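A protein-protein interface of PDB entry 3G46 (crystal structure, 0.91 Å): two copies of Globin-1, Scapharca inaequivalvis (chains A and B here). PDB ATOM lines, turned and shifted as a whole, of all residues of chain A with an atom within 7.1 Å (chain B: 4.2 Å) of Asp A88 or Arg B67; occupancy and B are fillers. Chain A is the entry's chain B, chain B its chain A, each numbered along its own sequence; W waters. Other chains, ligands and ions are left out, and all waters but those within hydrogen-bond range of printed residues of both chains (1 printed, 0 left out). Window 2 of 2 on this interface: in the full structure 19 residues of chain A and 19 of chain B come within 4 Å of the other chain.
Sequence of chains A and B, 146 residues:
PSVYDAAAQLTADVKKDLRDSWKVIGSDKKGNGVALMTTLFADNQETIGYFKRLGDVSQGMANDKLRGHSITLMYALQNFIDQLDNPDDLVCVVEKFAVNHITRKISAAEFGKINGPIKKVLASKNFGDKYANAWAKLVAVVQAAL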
ATOM      1  N   TYR A   4     -28.757  28.595  -6.096  1.00  0.00           N
ATOM      2  CA  TYR A   4     -28.457  27.508  -7.022  1.00  0.00           C
ATOM      3  C   TYR A   4     -28.179  28.032  -8.429  1.00  0.00           C
ATOM      4  O   TYR A   4     -27.268  27.560  -9.106  1.00  0.00           O
ATOM      5  CB  TYR A   4     -29.598  26.491  -7.086  1.00  0.00           C
ATOM      6  CG  TYR A   4     -29.679  25.512  -5.941  1.00  0.00           C
ATOM      7  CD1 TYR A   4     -30.404  25.790  -4.784  1.00  0.00           C
ATOM      8  CD2 TYR A   4     -29.024  24.282  -5.992  1.00  0.00           C
ATOM      9  CE1 TYR A   4     -30.452  24.863  -3.752  1.00  0.00           C
ATOM     10  CE2 TYR A   4     -29.070  23.357  -4.967  1.00  0.00           C
ATOM     11  CZ  TYR A   4     -29.799  23.660  -3.832  1.00  0.00           C
ATOM     12  OH  TYR A   4     -29.857  22.748  -2.796  1.00  0.00           O
ATOM     13  N   GLN A  83     -17.120  21.673  -1.191  1.00  0.00           N
ATOM     14  CA  GLN A  83     -18.502  21.401  -1.572  1.00  0.00           C
ATOM     15  C   GLN A  83     -18.801  21.679  -3.045  1.00  0.00           C
ATOM     16  O   GLN A  83     -19.962  21.524  -3.440  1.00  0.00           O
ATOM     17  CB  GLN A  83     -19.469  22.229  -0.725  1.00  0.00           C
ATOM     18  CG  GLN A  83     -19.338  22.209   0.772  1.00  0.00           C
ATOM     19  CD  GLN A  83     -18.859  20.917   1.396  1.00  0.00           C
ATOM     20  OE1 GLN A  83     -18.003  20.966   2.311  1.00  0.00           O
ATOM     21  NE2 GLN A  83     -19.389  19.807   0.939  1.00  0.00           N
ATOM     22  N   ASP A  85     -18.698  20.322  -5.902  1.00  0.00           N
ATOM     23  CA  ASP A  85     -19.340  19.387  -6.833  1.00  0.00           C
ATOM     24  C   ASP A  85     -20.758  19.030  -6.417  1.00  0.00           C
ATOM     25  O   ASP A  85     -21.463  18.334  -7.169  1.00  0.00           O
ATOM     26  CB  ASP A  85     -18.488  18.117  -6.957  1.00  0.00           C
ATOM     27  CG  ASP A  85     -17.246  18.356  -7.790  1.00  0.00           C
ATOM     28  OD1 ASP A  85     -17.216  19.250  -8.656  1.00  0.00           O
ATOM     29  OD2 ASP A  85     -16.244  17.636  -7.574  1.00  0.00           O
ATOM     30  N   ASN A  86     -21.196  19.476  -5.251  1.00  0.00           N
ATOM     31  CA  ASN A  86     -22.544  19.196  -4.770  1.00  0.00           C
ATOM     32  C   ASN A  86     -23.213  20.511  -4.415  1.00  0.00           C
ATOM     33  O   ASN A  86     -23.123  20.998  -3.286  1.00  0.00           O
ATOM     34  CB  ASN A  86     -22.507  18.237  -3.591  1.00  0.00           C
ATOM     35  CG  ASN A  86     -23.895  17.775  -3.191  1.00  0.00           C
ATOM     36  OD1 ASN A  86     -24.843  18.555  -3.216  1.00  0.00           O
ATOM     37  ND2 ASN A  86     -23.995  16.504  -2.828  1.00  0.00           N
ATOM     38  N   PRO A  87     -23.879  21.110  -5.386  1.00  0.00           N
ATOM     39  CA  PRO A  87     -24.588  22.372  -5.120  1.00  0.00           C
ATOM     40  C   PRO A  87     -25.521  22.310  -3.912  1.00  0.00           C
ATOM     41  O   PRO A  87     -25.649  23.349  -3.245  1.00  0.00           O
ATOM     42  CB  PRO A  87     -25.380  22.586  -6.426  1.00  0.00           C
ATOM     43  CG  PRO A  87     -24.510  21.938  -7.459  1.00  0.00           C
ATOM     44  CD  PRO A  87     -23.996  20.690  -6.793  1.00  0.00           C
ATOM     45  N   ASP A  88     -26.172  21.201  -3.577  1.00  0.00           N
ATOM     46  CA  ASP A  88     -26.982  21.172  -2.363  1.00  0.00           C
ATOM     47  C   ASP A  88     -26.157  21.485  -1.121  1.00  0.00           C
ATOM     48  O   ASP A  88     -26.551  22.228  -0.221  1.00  0.00           O
ATOM     49  CB  ASP A  88     -27.638  19.803  -2.171  1.00  0.00           C
ATOM     50  CG  ASP A  88     -28.648  19.438  -3.233  1.00  0.00           C
ATOM     51  OD1 ASP A  88     -29.418  20.336  -3.636  1.00  0.00           O
ATOM     52  OD2 ASP A  88     -28.684  18.266  -3.666  1.00  0.00           O
ATOM     53  N   ASP A  89     -24.970  20.898  -1.059  1.00  0.00           N
ATOM     54  CA  ASP A  89     -24.108  21.121   0.104  1.00  0.00           C
ATOM     55  C   ASP A  89     -23.482  22.509   0.048  1.00  0.00           C
ATOM     56  O   ASP A  89     -23.380  23.205   1.065  1.00  0.00           O
ATOM     57  CB  ASP A  89     -23.050  20.030   0.167  1.00  0.00           C
ATOM     58  CG  ASP A  89     -23.641  18.684   0.543  1.00  0.00           C
ATOM     59  OD1 ASP A  89     -24.787  18.632   1.050  1.00  0.00           O
ATOM     60  OD2 ASP A  89     -22.936  17.677   0.325  1.00  0.00           O
ATOM     61  N   LEU A  90     -23.052  22.950  -1.130  1.00  0.00           N
ATOM     62  CA  LEU A  90     -22.500  24.298  -1.233  1.00  0.00           C
ATOM     63  C   LEU A  90     -23.520  25.331  -0.794  1.00  0.00           C
ATOM     64  O   LEU A  90     -23.188  26.253  -0.027  1.00  0.00           O
ATOM     65  CB  LEU A  90     -22.033  24.596  -2.664  1.00  0.00           C
ATOM     66  CG  LEU A  90     -21.410  25.982  -2.851  1.00  0.00           C
ATOM     67  CD1 LEU A  90     -20.152  26.167  -2.019  1.00  0.00           C
ATOM     68  CD2 LEU A  90     -21.112  26.224  -4.333  1.00  0.00           C
ATOM     69  N   VAL A  91     -24.753  25.206  -1.270  1.00  0.00           N
ATOM     70  CA  VAL A  91     -25.753  26.218  -0.939  1.00  0.00           C
ATOM     71  C   VAL A  91     -25.988  26.235   0.564  1.00  0.00           C
ATOM     72  O   VAL A  91     -26.097  27.321   1.142  1.00  0.00           O
ATOM     73  CB  VAL A  91     -27.072  25.978  -1.701  1.00  0.00           C
ATOM     74  CG1 VAL A  91     -28.201  26.852  -1.192  1.00  0.00           C
ATOM     75  CG2 VAL A  91     -26.830  26.222  -3.178  1.00  0.00           C
ATOM     76  N   CYS A  92     -26.076  25.078   1.220  1.00  0.00           N
ATOM     77  CA  CYS A  92     -26.431  25.142   2.653  1.00  0.00           C
ATOM     78  C   CYS A  92     -25.268  25.746   3.462  1.00  0.00           C
ATOM     79  O   CYS A  92     -25.538  26.420   4.472  1.00  0.00           O
ATOM     80  CB  CYS A  92     -26.868  23.781   3.168  1.00  0.00           C
ATOM     81  SG  CYS A  92     -25.658  22.510   3.472  1.00  0.00           S
ATOM     82  N   VAL A  93     -24.013  25.546   3.063  1.00  0.00           N
ATOM     83  CA  VAL A  93     -22.922  26.183   3.831  1.00  0.00           C
ATOM     84  C   VAL A  93     -22.820  27.655   3.447  1.00  0.00           C
ATOM     85  O   VAL A  93     -22.548  28.501   4.318  1.00  0.00           O
ATOM     86  CB  VAL A  93     -21.551  25.480   3.690  1.00  0.00           C
ATOM     87  CG1 VAL A  93     -21.666  24.039   4.212  1.00  0.00           C
ATOM     88  CG2 VAL A  93     -21.012  25.428   2.285  1.00  0.00           C
ATOM     89  N   LYS B  30     -19.823  15.655   6.319  1.00  0.00           N
ATOM     90  CA  LYS B  30     -21.278  15.765   6.302  1.00  0.00           C
ATOM     91  C   LYS B  30     -21.941  14.697   7.152  1.00  0.00           C
ATOM     92  O   LYS B  30     -22.758  14.944   8.039  1.00  0.00           O
ATOM     93  CB  LYS B  30     -21.765  15.679   4.852  1.00  0.00           C
ATOM     94  CG  LYS B  30     -23.274  15.614   4.706  1.00  0.00           C
ATOM     95  CD  LYS B  30     -23.719  15.851   3.283  1.00  0.00           C
ATOM     96  CE  LYS B  30     -23.183  14.830   2.299  1.00  0.00           C
ATOM     97  NZ  LYS B  30     -23.705  15.038   0.920  1.00  0.00           N
ATOM     98  N   MET B  61     -30.410  14.991   8.350  1.00  0.00           N
ATOM     99  CA  MET B  61     -29.692  15.317   7.123  1.00  0.00           C
ATOM    100  C   MET B  61     -30.532  16.080   6.110  1.00  0.00           C
ATOM    101  O   MET B  61     -30.022  16.821   5.267  1.00  0.00           O
ATOM    102  CB  MET B  61     -29.183  14.003   6.508  1.00  0.00           C
ATOM    103  CG  MET B  61     -28.306  14.171   5.280  1.00  0.00           C
ATOM    104  SD  MET B  61     -26.690  14.857   5.644  1.00  0.00           S
ATOM    105  CE  MET B  61     -25.896  13.509   6.514  1.00  0.00           C
ATOM    106  N   ASN B  63     -32.621  18.383   6.794  1.00  0.00           N
ATOM    107  CA  ASN B  63     -32.706  19.781   7.196  1.00  0.00           C
ATOM    108  C   ASN B  63     -31.475  20.532   6.709  1.00  0.00           C
ATOM    109  O   ASN B  63     -30.372  20.332   7.217  1.00  0.00           O
ATOM    110  CB  ASN B  63     -32.864  19.862   8.712  1.00  0.00           C
ATOM    111  CG  ASN B  63     -32.890  21.252   9.304  1.00  0.00           C
ATOM    112  OD1 ASN B  63     -32.303  22.200   8.789  1.00  0.00           O
ATOM    113  ND2 ASN B  63     -33.583  21.414  10.429  1.00  0.00           N
ATOM    114  N   ASP B  64     -31.658  21.397   5.720  1.00  0.00           N
ATOM    115  CA  ASP B  64     -30.552  22.085   5.070  1.00  0.00           C
ATOM    116  C   ASP B  64     -29.757  22.947   6.045  1.00  0.00           C
ATOM    117  O   ASP B  64     -28.529  22.966   6.016  1.00  0.00           O
ATOM    118  CB  ASP B  64     -31.064  22.962   3.919  1.00  0.00           C
ATOM    119  CG  ASP B  64     -31.730  22.184   2.805  1.00  0.00           C
ATOM    120  OD1 ASP B  64     -31.268  21.082   2.448  1.00  0.00           O
ATOM    121  OD2 ASP B  64     -32.733  22.709   2.287  1.00  0.00           O
ATOM    122  N   LYS B  65     -30.451  23.683   6.925  1.00  0.00           N
ATOM    123  CA  LYS B  65     -29.704  24.515   7.878  1.00  0.00           C
ATOM    124  C   LYS B  65     -28.924  23.628   8.843  1.00  0.00           C
ATOM    125  O   LYS B  65     -27.787  23.952   9.193  1.00  0.00           O
ATOM    126  CB  LYS B  65     -30.626  25.449   8.654  1.00  0.00           C
ATOM    127  CG  LYS B  65     -31.224  26.561   7.814  1.00  0.00           C
ATOM    128  CD  LYS B  65     -32.068  27.477   8.679  1.00  0.00           C
ATOM    129  CE  LYS B  65     -32.546  28.695   7.916  1.00  0.00           C
ATOM    130  NZ  LYS B  65     -33.418  28.359   6.761  1.00  0.00           N
ATOM    131  N   LEU B  66     -29.506  22.526   9.280  1.00  0.00           N
ATOM    132  CA  LEU B  66     -28.729  21.641  10.152  1.00  0.00           C
ATOM    133  C   LEU B  66     -27.538  21.055   9.406  1.00  0.00           C
ATOM    134  O   LEU B  66     -26.446  20.939   9.975  1.00  0.00           O
ATOM    135  CB  LEU B  66     -29.612  20.531  10.709  1.00  0.00           C
ATOM    136  CG  LEU B  66     -28.915  19.503  11.600  1.00  0.00           C
ATOM    137  CD1 LEU B  66     -28.226  20.149  12.796  1.00  0.00           C
ATOM    138  CD2 LEU B  66     -29.943  18.479  12.048  1.00  0.00           C
ATOM    139  N   ARG B  67     -27.740  20.682   8.139  1.00  0.00           N
ATOM    140  CA  ARG B  67     -26.615  20.129   7.378  1.00  0.00           C
ATOM    141  C   ARG B  67     -25.505  21.165   7.217  1.00  0.00           C
ATOM    142  O   ARG B  67     -24.326  20.854   7.385  1.00  0.00           O
ATOM    143  CB  ARG B  67     -27.103  19.608   6.017  1.00  0.00           C
ATOM    144  CG  ARG B  67     -26.105  18.700   5.319  1.00  0.00           C
ATOM    145  CD  ARG B  67     -26.700  18.019   4.094  1.00  0.00           C
ATOM    146  NE  ARG B  67     -27.000  19.005   3.053  1.00  0.00           N
ATOM    147  CZ  ARG B  67     -28.198  19.476   2.757  1.00  0.00           C
ATOM    148  NH1 ARG B  67     -29.300  19.097   3.383  1.00  0.00           N
ATOM    149  NH2 ARG B  67     -28.303  20.378   1.779  1.00  0.00           N
ATOM    150  N   GLY B  68     -25.846  22.411   6.887  1.00  0.00           N
ATOM    151  CA  GLY B  68     -24.856  23.466   6.737  1.00  0.00           C
ATOM    152  C   GLY B  68     -24.098  23.738   8.026  1.00  0.00           C
ATOM    153  O   GLY B  68     -22.885  23.897   8.048  1.00  0.00           O
ATOM    154  N   HIS B  69     -24.843  23.791   9.133  1.00  0.00           N
ATOM    155  CA  HIS B  69     -24.258  23.942  10.450  1.00  0.00           C
ATOM    156  C   HIS B  69     -23.273  22.818  10.752  1.00  0.00           C
ATOM    157  O   HIS B  69     -22.167  23.015  11.249  1.00  0.00           O
ATOM    158  CB  HIS B  69     -25.376  23.999  11.511  1.00  0.00           C
ATOM    159  CG  HIS B  69     -24.838  23.786  12.884  1.00  0.00           C
ATOM    160  ND1 HIS B  69     -24.302  24.809  13.633  1.00  0.00           N
ATOM    161  CD2 HIS B  69     -24.762  22.649  13.625  1.00  0.00           C
ATOM    162  CE1 HIS B  69     -23.920  24.274  14.779  1.00  0.00           C
ATOM    163  NE2 HIS B  69     -24.186  22.972  14.804  1.00  0.00           N
ATOM    164  N   SER B  70     -23.708  21.584  10.467  1.00  0.00           N
ATOM    165  CA  SER B  70     -22.965  20.403  10.854  1.00  0.00           C
ATOM    166  C   SER B  70     -21.660  20.253  10.068  1.00  0.00           C
ATOM    167  O   SER B  70     -20.616  19.929  10.617  1.00  0.00           O
ATOM    168  CB  SER B  70     -23.805  19.142  10.648  1.00  0.00           C
ATOM    169  OG  SER B  70     -24.995  19.138  11.368  1.00  0.00           O
ATOM    170  N   ILE B  71     -21.754  20.498   8.766  1.00  0.00           N
ATOM    171  CA  ILE B  71     -20.535  20.527   7.950  1.00  0.00           C
ATOM    172  C   ILE B  71     -19.566  21.574   8.488  1.00  0.00           C
ATOM    173  O   ILE B  71     -18.372  21.327   8.649  1.00  0.00           O
ATOM    174  CB  ILE B  71     -20.877  20.771   6.467  1.00  0.00           C
ATOM    175  CG1 ILE B  71     -21.685  19.640   5.839  1.00  0.00           C
ATOM    176  CG2 ILE B  71     -19.617  21.043   5.666  1.00  0.00           C
ATOM    177  CD1 ILE B  71     -22.359  19.973   4.529  1.00  0.00           C
HETATM  178  O   HOH W   1     -29.167  23.138   0.206  1.00  0.00           O
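The guanidinium group of Arg B67 sits at hydrogen-bond distance from the backbone carbonyl oxygen of Asp A88 (3.2 Å).
The side-chain carboxylate (OD1) of Asp A89 is in salt-bridge range of the guanidinium group (NE) of Arg B67 (3.0 Å).
SG of Cys A92 is in hydrogen-bond range of NE of Arg B67 (3.8 Å).
The side-chain carboxylate (OD2) of Asp A89 lies within salt-bridge range of the side-chain amino group (NZ) of Lys B30 (2.8 Å).
The side-chain sulfur (SG) of Cys A92 is in hydrogen-bond range of the backbone NH (N) of Gly B68 (3.4 Å).
The backbone carbonyl oxygen (O) of Asp A89 sits at hydrogen-bond distance from the side-chain sulfur (SG) of Cys A92, at 3.4 Å.
The side-chain amide oxygen (OD1) of Asn A86 lies within hydrogen-bond range of the backbone NH (N) of Asp A89 (3.2 Å).
The side-chain amide oxygen (OD1) of Asn A86 lies within hydrogen-bond range of the backbone NH (N) of Asp A88.
The side-chain hydroxyl of Tyr A4 lies within hydrogen-bond range of the side-chain carboxylate of Asp A88 (2.6 Å).
The backbone carbonyl oxygen (O) of Met B61 sits at hydrogen-bond distance from the guanidinium group (NH1) of Arg B67.
OD1 of Asp B64 lies within salt-bridge range of NH1 of Arg B67, at 2.9 Å.
Among the printed residues, pairs that only touch across the chains: Gln A83 with Ile B71, Cys A92 with Asp B64 and Val A93 with Ile B71.
Printed residues of chain B within 4 Å of Asp A88: Arg B67.
Of the printed residues of chain B, Asp A89 touches Lys B30 and Arg B67.
Printed residues of chain B within 4 Å of Val A93: Ile B71 (3.9 Å).
Of the printed residues of chain A, Lys B30 touches Asp A89.
Asn B63 touches none of the printed residues of chain A.
Printed residues of chain A within 4 Å of Asp B64: Cys A92 (3.4 Å).
Of chain A, only Asp A88, Asp A89 and Cys A92 come within 4 Å of Arg B67.
Printed residues of chain A within 4 Å of Ile B71: Gln A83 (3.7 Å) and Val A93 (3.9 Å).
The nearest printed residue of chain A that does not touch Ile B71 is Cys A92 (4.3 Å).
Of the 11 printed residues of chain A, 5 touch a printed residue of chain B.
Hydrophobic or aromatic side chains of chain A within 4 Å of the printed part of chain B: Val A93.
Of the 11 printed residues of chain B, 5 touch a printed residue of chain A.
Printed residues of chain B that touch a printed residue of chain A: Lys B30, Asp B64, Arg B67, Gly B68 and Ile B71.
Hydrophobic or aromatic side chains of chain B within 4 Å of the printed part of chain A: Ile B71.
Among the printed residues, Asp or Glu carboxylates within 4 Å of a Lys or Arg side-chain nitrogen of the other chain: Asp A89 with Lys B30 (2.8 Å) and Asp A89 with Arg B67 (3.0 Å).
No position is printed for both chains.
Of the 8 pairs that touch across the chains among the printed residues, none has its exchanged pair printed and touching as well.
Water W1 lies within hydrogen-bond range of O of Asp A88 (2.8 Å), OH of Tyr A4 (3.1 Å) and NH2 of Arg B67 (3.3 Å).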
